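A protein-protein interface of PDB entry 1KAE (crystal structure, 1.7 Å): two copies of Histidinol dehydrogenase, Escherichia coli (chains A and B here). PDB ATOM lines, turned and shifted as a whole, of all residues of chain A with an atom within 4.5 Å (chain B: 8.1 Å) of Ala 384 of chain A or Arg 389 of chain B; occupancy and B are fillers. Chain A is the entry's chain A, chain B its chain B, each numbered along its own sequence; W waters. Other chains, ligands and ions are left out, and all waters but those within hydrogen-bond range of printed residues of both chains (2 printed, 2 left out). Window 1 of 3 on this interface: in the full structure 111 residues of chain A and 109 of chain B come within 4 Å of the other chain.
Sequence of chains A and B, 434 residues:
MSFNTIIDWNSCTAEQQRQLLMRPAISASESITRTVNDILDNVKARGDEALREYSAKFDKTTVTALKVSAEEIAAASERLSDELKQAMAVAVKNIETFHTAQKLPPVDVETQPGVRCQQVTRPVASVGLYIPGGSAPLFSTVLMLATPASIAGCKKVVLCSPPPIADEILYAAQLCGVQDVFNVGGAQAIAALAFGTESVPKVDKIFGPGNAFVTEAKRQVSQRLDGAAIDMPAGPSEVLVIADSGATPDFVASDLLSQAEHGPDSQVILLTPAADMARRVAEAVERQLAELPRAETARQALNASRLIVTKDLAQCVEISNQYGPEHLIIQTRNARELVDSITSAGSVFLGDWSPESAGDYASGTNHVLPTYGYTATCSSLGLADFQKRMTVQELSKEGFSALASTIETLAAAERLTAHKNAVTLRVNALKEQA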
ATOM      1  N   SER A 379     -25.761 -26.825 -10.165  1.00  0.00           N
ATOM      2  CA  SER A 379     -24.717 -26.607 -11.142  1.00  0.00           C
ATOM      3  C   SER A 379     -24.867 -25.317 -11.931  1.00  0.00           C
ATOM      4  O   SER A 379     -25.946 -24.751 -12.069  1.00  0.00           O
ATOM      5  CB  SER A 379     -24.762 -27.722 -12.212  1.00  0.00           C
ATOM      6  OG  SER A 379     -24.570 -29.014 -11.660  1.00  0.00           O
ATOM      7  N   SER A 380     -23.742 -24.887 -12.476  1.00  0.00           N
ATOM      8  CA  SER A 380     -23.689 -23.811 -13.433  1.00  0.00           C
ATOM      9  C   SER A 380     -24.580 -24.366 -14.540  1.00  0.00           C
ATOM     10  O   SER A 380     -24.702 -25.610 -14.689  1.00  0.00           O
ATOM     11  CB  SER A 380     -22.256 -23.711 -14.005  1.00  0.00           C
ATOM     12  OG  SER A 380     -22.267 -23.097 -15.309  1.00  0.00           O
ATOM     13  N   LEU A 381     -25.249 -23.491 -15.282  1.00  0.00           N
ATOM     14  CA  LEU A 381     -26.043 -23.953 -16.406  1.00  0.00           C
ATOM     15  C   LEU A 381     -24.983 -24.556 -17.354  1.00  0.00           C
ATOM     16  O   LEU A 381     -23.850 -24.067 -17.417  1.00  0.00           O
ATOM     17  CB  LEU A 381     -26.723 -22.807 -17.137  1.00  0.00           C
ATOM     18  CG  LEU A 381     -27.778 -23.223 -18.169  1.00  0.00           C
ATOM     19  CD1 LEU A 381     -29.055 -23.697 -17.411  1.00  0.00           C
ATOM     20  CD2 LEU A 381     -28.107 -22.044 -19.092  1.00  0.00           C
ATOM     21  N   GLY A 382     -25.357 -25.574 -18.104  1.00  0.00           N
ATOM     22  CA  GLY A 382     -24.411 -26.208 -19.019  1.00  0.00           C
ATOM     23  C   GLY A 382     -25.236 -27.062 -19.946  1.00  0.00           C
ATOM     24  O   GLY A 382     -26.461 -27.029 -19.926  1.00  0.00           O
ATOM     25  N   LEU A 383     -24.574 -27.845 -20.777  1.00  0.00           N
ATOM     26  CA  LEU A 383     -25.290 -28.699 -21.707  1.00  0.00           C
ATOM     27  C   LEU A 383     -26.315 -29.642 -21.053  1.00  0.00           C
ATOM     28  O   LEU A 383     -27.412 -29.895 -21.617  1.00  0.00           O
ATOM     29  CB  LEU A 383     -24.285 -29.530 -22.474  1.00  0.00           C
ATOM     30  CG  LEU A 383     -24.838 -30.351 -23.630  1.00  0.00           C
ATOM     31  CD1 LEU A 383     -25.237 -29.413 -24.781  1.00  0.00           C
ATOM     32  CD2 LEU A 383     -23.735 -31.358 -24.082  1.00  0.00           C
ATOM     33  N   ALA A 384     -25.983 -30.147 -19.873  1.00  0.00           N
ATOM     34  CA  ALA A 384     -26.833 -31.132 -19.214  1.00  0.00           C
ATOM     35  C   ALA A 384     -28.232 -30.577 -18.880  1.00  0.00           C
ATOM     36  O   ALA A 384     -29.196 -31.353 -18.760  1.00  0.00           O
ATOM     37  CB  ALA A 384     -26.133 -31.656 -17.945  1.00  0.00           C
ATOM     38  N   ASP A 385     -28.349 -29.255 -18.722  1.00  0.00           N
ATOM     39  CA  ASP A 385     -29.638 -28.664 -18.401  1.00  0.00           C
ATOM     40  C   ASP A 385     -30.580 -28.629 -19.580  1.00  0.00           C
ATOM     41  O   ASP A 385     -31.761 -28.321 -19.431  1.00  0.00           O
ATOM     42  CB  ASP A 385     -29.456 -27.258 -17.819  1.00  0.00           C
ATOM     43  CG  ASP A 385     -28.646 -27.280 -16.541  1.00  0.00           C
ATOM     44  OD1 ASP A 385     -29.196 -27.684 -15.482  1.00  0.00           O
ATOM     45  OD2 ASP A 385     -27.452 -26.937 -16.597  1.00  0.00           O
ATOM     46  N   PHE A 386     -30.091 -28.993 -20.750  1.00  0.00           N
ATOM     47  CA  PHE A 386     -30.952 -29.016 -21.930  1.00  0.00           C
ATOM     48  C   PHE A 386     -31.203 -30.450 -22.421  1.00  0.00           C
ATOM     49  O   PHE A 386     -31.693 -30.664 -23.537  1.00  0.00           O
ATOM     50  CB  PHE A 386     -30.318 -28.199 -23.059  1.00  0.00           C
ATOM     51  CG  PHE A 386     -30.183 -26.729 -22.735  1.00  0.00           C
ATOM     52  CD1 PHE A 386     -29.080 -26.246 -22.015  1.00  0.00           C
ATOM     53  CD2 PHE A 386     -31.194 -25.829 -23.109  1.00  0.00           C
ATOM     54  CE1 PHE A 386     -28.987 -24.877 -21.672  1.00  0.00           C
ATOM     55  CE2 PHE A 386     -31.099 -24.452 -22.758  1.00  0.00           C
ATOM     56  CZ  PHE A 386     -30.000 -23.998 -22.044  1.00  0.00           C
ATOM     57  N   GLN A 387     -30.877 -31.421 -21.577  1.00  0.00           N
ATOM     58  CA  GLN A 387     -31.068 -32.810 -21.937  1.00  0.00           C
ATOM     59  C   GLN A 387     -31.388 -33.645 -20.716  1.00  0.00           C
ATOM     60  O   GLN A 387     -31.536 -33.105 -19.601  1.00  0.00           O
ATOM     61  CB  GLN A 387     -29.821 -33.325 -22.684  1.00  0.00           C
ATOM     62  CG  GLN A 387     -28.547 -33.259 -21.955  1.00  0.00           C
ATOM     63  CD  GLN A 387     -27.340 -33.595 -22.870  1.00  0.00           C
ATOM     64  OE1 GLN A 387     -26.303 -34.037 -22.399  1.00  0.00           O
ATOM     65  NE2 GLN A 387     -27.493 -33.381 -24.151  1.00  0.00           N
ATOM     66  N   LEU B 104     -17.939 -38.300 -14.927  1.00  0.00           N
ATOM     67  CA  LEU B 104     -17.722 -37.401 -16.071  1.00  0.00           C
ATOM     68  C   LEU B 104     -16.235 -37.334 -16.441  1.00  0.00           C
ATOM     69  O   LEU B 104     -15.372 -37.250 -15.568  1.00  0.00           O
ATOM     70  CB  LEU B 104     -18.222 -35.985 -15.770  1.00  0.00           C
ATOM     71  CG  LEU B 104     -19.705 -35.716 -15.454  1.00  0.00           C
ATOM     72  CD1 LEU B 104     -19.943 -34.221 -15.412  1.00  0.00           C
ATOM     73  CD2 LEU B 104     -20.608 -36.305 -16.500  1.00  0.00           C
ATOM     74  N   VAL B 107     -13.206 -31.980 -18.476  1.00  0.00           N
ATOM     75  CA  VAL B 107     -13.591 -31.053 -19.529  1.00  0.00           C
ATOM     76  C   VAL B 107     -12.556 -29.948 -19.356  1.00  0.00           C
ATOM     77  O   VAL B 107     -12.560 -29.230 -18.340  1.00  0.00           O
ATOM     78  CB  VAL B 107     -15.032 -30.529 -19.324  1.00  0.00           C
ATOM     79  CG1 VAL B 107     -15.351 -29.447 -20.366  1.00  0.00           C
ATOM     80  CG2 VAL B 107     -15.999 -31.669 -19.504  1.00  0.00           C
ATOM     81  N   GLN B 118     -12.632 -24.910 -18.007  1.00  0.00           N
ATOM     82  CA  GLN B 118     -12.844 -26.260 -17.525  1.00  0.00           C
ATOM     83  C   GLN B 118     -14.184 -26.376 -16.825  1.00  0.00           C
ATOM     84  O   GLN B 118     -14.738 -25.388 -16.346  1.00  0.00           O
ATOM     85  CB  GLN B 118     -11.802 -26.622 -16.493  1.00  0.00           C
ATOM     86  CG  GLN B 118     -10.342 -26.547 -16.934  1.00  0.00           C
ATOM     87  CD  GLN B 118      -9.444 -26.631 -15.727  1.00  0.00           C
ATOM     88  OE1 GLN B 118      -9.035 -27.726 -15.308  1.00  0.00           O
ATOM     89  NE2 GLN B 118      -9.165 -25.482 -15.123  1.00  0.00           N
ATOM     90  N   GLN B 119     -14.667 -27.609 -16.740  1.00  0.00           N
ATOM     91  CA  GLN B 119     -15.868 -27.943 -15.997  1.00  0.00           C
ATOM     92  C   GLN B 119     -15.425 -29.029 -15.035  1.00  0.00           C
ATOM     93  O   GLN B 119     -14.904 -30.049 -15.449  1.00  0.00           O
ATOM     94  CB  GLN B 119     -16.930 -28.528 -16.905  1.00  0.00           C
ATOM     95  CG  GLN B 119     -18.199 -28.993 -16.127  1.00  0.00           C
ATOM     96  CD  GLN B 119     -19.132 -29.796 -17.012  1.00  0.00           C
ATOM     97  OE1 GLN B 119     -19.041 -31.044 -17.071  1.00  0.00           O
ATOM     98  NE2 GLN B 119     -20.003 -29.115 -17.735  1.00  0.00           N
ATOM     99  N   VAL B 120     -15.618 -28.846 -13.740  1.00  0.00           N
ATOM    100  CA  VAL B 120     -15.205 -29.866 -12.820  1.00  0.00           C
ATOM    101  C   VAL B 120     -16.443 -30.193 -12.013  1.00  0.00           C
ATOM    102  O   VAL B 120     -17.436 -29.469 -12.113  1.00  0.00           O
ATOM    103  CB  VAL B 120     -14.084 -29.389 -11.881  1.00  0.00           C
ATOM    104  CG1 VAL B 120     -12.827 -29.110 -12.680  1.00  0.00           C
ATOM    105  CG2 VAL B 120     -14.519 -28.123 -11.128  1.00  0.00           C
ATOM    106  N   THR B 121     -16.407 -31.274 -11.250  1.00  0.00           N
ATOM    107  CA  THR B 121     -17.563 -31.637 -10.444  1.00  0.00           C
ATOM    108  C   THR B 121     -17.173 -31.645  -8.988  1.00  0.00           C
ATOM    109  O   THR B 121     -16.011 -31.859  -8.641  1.00  0.00           O
ATOM    110  CB  THR B 121     -18.092 -33.031 -10.820  1.00  0.00           C
ATOM    111  OG1 THR B 121     -17.063 -34.005 -10.603  1.00  0.00           O
ATOM    112  CG2 THR B 121     -18.543 -33.053 -12.281  1.00  0.00           C
ATOM    113  N   ARG B 122     -18.146 -31.406  -8.115  1.00  0.00           N
ATOM    114  CA  ARG B 122     -17.926 -31.400  -6.677  1.00  0.00           C
ATOM    115  C   ARG B 122     -19.140 -32.122  -6.128  1.00  0.00           C
ATOM    116  O   ARG B 122     -20.256 -31.949  -6.629  1.00  0.00           O
ATOM    117  CB  ARG B 122     -17.850 -29.951  -6.122  1.00  0.00           C
ATOM    118  CG  ARG B 122     -16.625 -29.157  -6.658  1.00  0.00           C
ATOM    119  CD  ARG B 122     -15.332 -29.789  -6.083  1.00  0.00           C
ATOM    120  NE  ARG B 122     -14.169 -28.952  -6.357  1.00  0.00           N
ATOM    121  CZ  ARG B 122     -13.294 -29.153  -7.341  1.00  0.00           C
ATOM    122  NH1 ARG B 122     -13.436 -30.188  -8.184  1.00  0.00           N
ATOM    123  NH2 ARG B 122     -12.273 -28.300  -7.479  1.00  0.00           N
ATOM    124  N   PRO B 123     -18.936 -32.987  -5.137  1.00  0.00           N
ATOM    125  CA  PRO B 123     -20.017 -33.744  -4.533  1.00  0.00           C
ATOM    126  C   PRO B 123     -20.943 -32.869  -3.696  1.00  0.00           C
ATOM    127  O   PRO B 123     -20.526 -31.856  -3.141  1.00  0.00           O
ATOM    128  CB  PRO B 123     -19.260 -34.742  -3.644  1.00  0.00           C
ATOM    129  CG  PRO B 123     -18.126 -33.975  -3.186  1.00  0.00           C
ATOM    130  CD  PRO B 123     -17.659 -33.323  -4.487  1.00  0.00           C
ATOM    131  N   THR B 377     -38.432 -33.809 -18.805  1.00  0.00           N
ATOM    132  CA  THR B 377     -37.251 -33.007 -18.497  1.00  0.00           C
ATOM    133  C   THR B 377     -36.304 -33.566 -17.445  1.00  0.00           C
ATOM    134  O   THR B 377     -35.167 -33.066 -17.329  1.00  0.00           O
ATOM    135  CB  THR B 377     -37.646 -31.616 -17.995  1.00  0.00           C
ATOM    136  OG1 THR B 377     -38.538 -31.768 -16.876  1.00  0.00           O
ATOM    137  CG2 THR B 377     -38.360 -30.844 -19.092  1.00  0.00           C
ATOM    138  N   SER B 379     -34.137 -36.744 -15.334  1.00  0.00           N
ATOM    139  CA  SER B 379     -33.380 -37.948 -15.646  1.00  0.00           C
ATOM    140  C   SER B 379     -33.558 -39.001 -14.593  1.00  0.00           C
ATOM    141  O   SER B 379     -33.955 -38.739 -13.458  1.00  0.00           O
ATOM    142  CB  SER B 379     -31.857 -37.649 -15.659  1.00  0.00           C
ATOM    143  OG  SER B 379     -31.469 -36.632 -16.568  1.00  0.00           O
ATOM    144  N   ALA B 384     -24.858 -38.080 -11.273  1.00  0.00           N
ATOM    145  CA  ALA B 384     -24.981 -36.625 -11.411  1.00  0.00           C
ATOM    146  C   ALA B 384     -25.886 -35.984 -10.349  1.00  0.00           C
ATOM    147  O   ALA B 384     -25.711 -34.809 -10.008  1.00  0.00           O
ATOM    148  CB  ALA B 384     -25.485 -36.281 -12.820  1.00  0.00           C
ATOM    149  N   GLN B 387     -23.931 -34.739  -7.146  1.00  0.00           N
ATOM    150  CA  GLN B 387     -22.820 -33.817  -7.318  1.00  0.00           C
ATOM    151  C   GLN B 387     -23.255 -32.595  -8.113  1.00  0.00           C
ATOM    152  O   GLN B 387     -24.443 -32.451  -8.465  1.00  0.00           O
ATOM    153  CB  GLN B 387     -21.633 -34.566  -7.980  1.00  0.00           C
ATOM    154  CG  GLN B 387     -21.921 -35.226  -9.297  1.00  0.00           C
ATOM    155  CD  GLN B 387     -20.717 -36.014  -9.914  1.00  0.00           C
ATOM    156  OE1 GLN B 387     -20.554 -36.015 -11.127  1.00  0.00           O
ATOM    157  NE2 GLN B 387     -19.931 -36.677  -9.103  1.00  0.00           N
ATOM    158  N   LYS B 388     -22.338 -31.666  -8.376  1.00  0.00           N
ATOM    159  CA  LYS B 388     -22.696 -30.504  -9.167  1.00  0.00           C
ATOM    160  C   LYS B 388     -21.512 -30.058 -10.012  1.00  0.00           C
ATOM    161  O   LYS B 388     -20.342 -30.271  -9.645  1.00  0.00           O
ATOM    162  CB  LYS B 388     -23.151 -29.325  -8.260  1.00  0.00           C
ATOM    163  CG  LYS B 388     -22.133 -28.826  -7.235  1.00  0.00           C
ATOM    164  CD  LYS B 388     -22.496 -29.288  -5.822  1.00  0.00           C
ATOM    165  CE  LYS B 388     -21.362 -29.008  -4.824  1.00  0.00           C
ATOM    166  NZ  LYS B 388     -21.160 -27.528  -4.496  1.00  0.00           N
ATOM    167  N   ARG B 389     -21.825 -29.462 -11.147  1.00  0.00           N
ATOM    168  CA  ARG B 389     -20.818 -28.968 -12.096  1.00  0.00           C
ATOM    169  C   ARG B 389     -20.422 -27.541 -11.748  1.00  0.00           C
ATOM    170  O   ARG B 389     -21.268 -26.714 -11.436  1.00  0.00           O
ATOM    171  CB  ARG B 389     -21.387 -29.009 -13.516  1.00  0.00           C
ATOM    172  CG  ARG B 389     -21.466 -30.412 -14.144  1.00  0.00           C
ATOM    173  CD  ARG B 389     -22.178 -30.404 -15.508  1.00  0.00           C
ATOM    174  NE  ARG B 389     -23.618 -30.189 -15.332  1.00  0.00           N
ATOM    175  CZ  ARG B 389     -24.270 -29.048 -15.559  1.00  0.00           C
ATOM    176  NH1 ARG B 389     -23.651 -27.939 -15.998  1.00  0.00           N
ATOM    177  NH2 ARG B 389     -25.575 -29.014 -15.315  1.00  0.00           N
ATOM    178  N   MET B 390     -19.126 -27.267 -11.762  1.00  0.00           N
ATOM    179  CA  MET B 390     -18.610 -25.941 -11.475  1.00  0.00           C
ATOM    180  C   MET B 390     -17.640 -25.607 -12.616  1.00  0.00           C
ATOM    181  O   MET B 390     -16.916 -26.493 -13.071  1.00  0.00           O
ATOM    182  CB  MET B 390     -17.928 -25.968 -10.112  1.00  0.00           C
ATOM    183  CG  MET B 390     -17.219 -24.687  -9.718  1.00  0.00           C
ATOM    184  SD  MET B 390     -16.559 -24.746  -7.923  1.00  0.00           S
ATOM    185  CE  MET B 390     -14.988 -25.929  -8.223  1.00  0.00           C
ATOM    186  N   THR B 391     -17.643 -24.370 -13.113  1.00  0.00           N
ATOM    187  CA  THR B 391     -16.724 -24.023 -14.193  1.00  0.00           C
ATOM    188  C   THR B 391     -15.554 -23.191 -13.691  1.00  0.00           C
ATOM    189  O   THR B 391     -15.593 -22.519 -12.612  1.00  0.00           O
ATOM    190  CB  THR B 391     -17.445 -23.320 -15.404  1.00  0.00           C
ATOM    191  OG1 THR B 391     -18.054 -22.097 -14.987  1.00  0.00           O
ATOM    192  CG2 THR B 391     -18.524 -24.250 -15.988  1.00  0.00           C
ATOM    193  N   VAL B 392     -14.481 -23.229 -14.460  1.00  0.00           N
ATOM    194  CA  VAL B 392     -13.253 -22.550 -14.077  1.00  0.00           C
ATOM    195  C   VAL B 392     -12.644 -21.983 -15.336  1.00  0.00           C
ATOM    196  O   VAL B 392     -12.728 -22.619 -16.400  1.00  0.00           O
ATOM    197  CB  VAL B 392     -12.225 -23.590 -13.447  1.00  0.00           C
ATOM    198  CG1 VAL B 392     -10.883 -22.910 -13.080  1.00  0.00           C
ATOM    199  CG2 VAL B 392     -12.840 -24.301 -12.237  1.00  0.00           C
HETATM  200  O   HOH W   1     -28.049 -30.411 -14.231  1.00  0.00           O
HETATM  201  O   HOH W   2     -20.288 -21.635 -16.255  1.00  0.00           O
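Water W2 lies within hydrogen-bond range of OG1 of Thr 391 of chain B (2.6 Å) and OG of Ser 380 of chain A (2.6 Å). Water W1 lies within hydrogen-bond range of NH2 of Arg 389 of chain B (3.0 Å) and OD1 of Asp 385 of chain A (3.2 Å).
Printed residues of chain B that touch a printed residue of chain A: Lys 388, Arg 389 and Thr 391. Hydrophobic or aromatic side chains of chain A that line the printed part of chain B: Ala 384. Among the printed residues, 8 pairs touch across the chains. Among the printed residues, Asp or Glu carboxylates within 4 Å of a Lys or Arg side-chain nitrogen of the other chain: Asp 385 of chain A with Arg 389 of chain B (3.1 Å).
The side-chain carboxylate (OD2) of Asp 385 of chain A is in salt-bridge range of the guanidinium group (NH2) of Arg 389 of chain B, at 3.1 Å. The backbone carbonyl oxygen (O) of Ser 380 of chain A is in hydrogen-bond range of the guanidinium group (NH1) of Arg 389 of chain B. OG of Ser 379 of chain A is in hydrogen-bond range of N of Arg 389 of chain B.
N of Gly 382 of chain A sits at hydrogen-bond distance from OD2 of Asp 385 of chain A (2.9 Å). O of Arg 122 of chain B is in hydrogen-bond range of N of Lys 388 of chain B, at 2.7 Å.
OG of Ser 379 of chain A touches CA of Lys 388 of chain B, at 3.5 Å. Ser 380 of chain A touches Thr 391 of chain B. Leu 381 of chain A touches Arg 389 of chain B. Arg 389 of chain B touches Gly 382 of chain A (NH1 to CA, 3.6 Å). Ala 384 of chain A touches Arg 389 of chain B (CB to NH2, 3.8 Å).
3 positions are printed for both chains. Of the 8 pairs that touch across the chains among the printed residues, none has its exchanged pair printed and touching as well.
Printed residues of chain B within 4 Å of Ser 379 of chain A: Lys 388 and Arg 389. Of the printed residues of chain B, Ser 380 of chain A touches Arg 389 and Thr 391. Gly 382 of chain A touches one residue of chain B. Ala 384 of chain A touches just one residue of chain B: Arg 389. Printed residues of chain A within 4 Å of Lys 388 of chain B: Ser 379. Arg 389 of chain B touches just these residues of chain A: Ser 379 (2.8 Å), Ser 380 (2.9 Å), Leu 381 (3.9 Å), Gly 382 (3.6 Å), Ala 384 (3.8 Å) and Asp 385 (3.1 Å). Of the printed residues of chain A, Thr 391 of chain B touches Ser 380. The nearest residue of chain B that does not touch Ala 384 of chain A is Ser 379 of chain B (6.2 Å). The nearest printed residue of chain A that does not touch Arg 389 of chain B is Leu 383 of chain A (4.9 Å).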
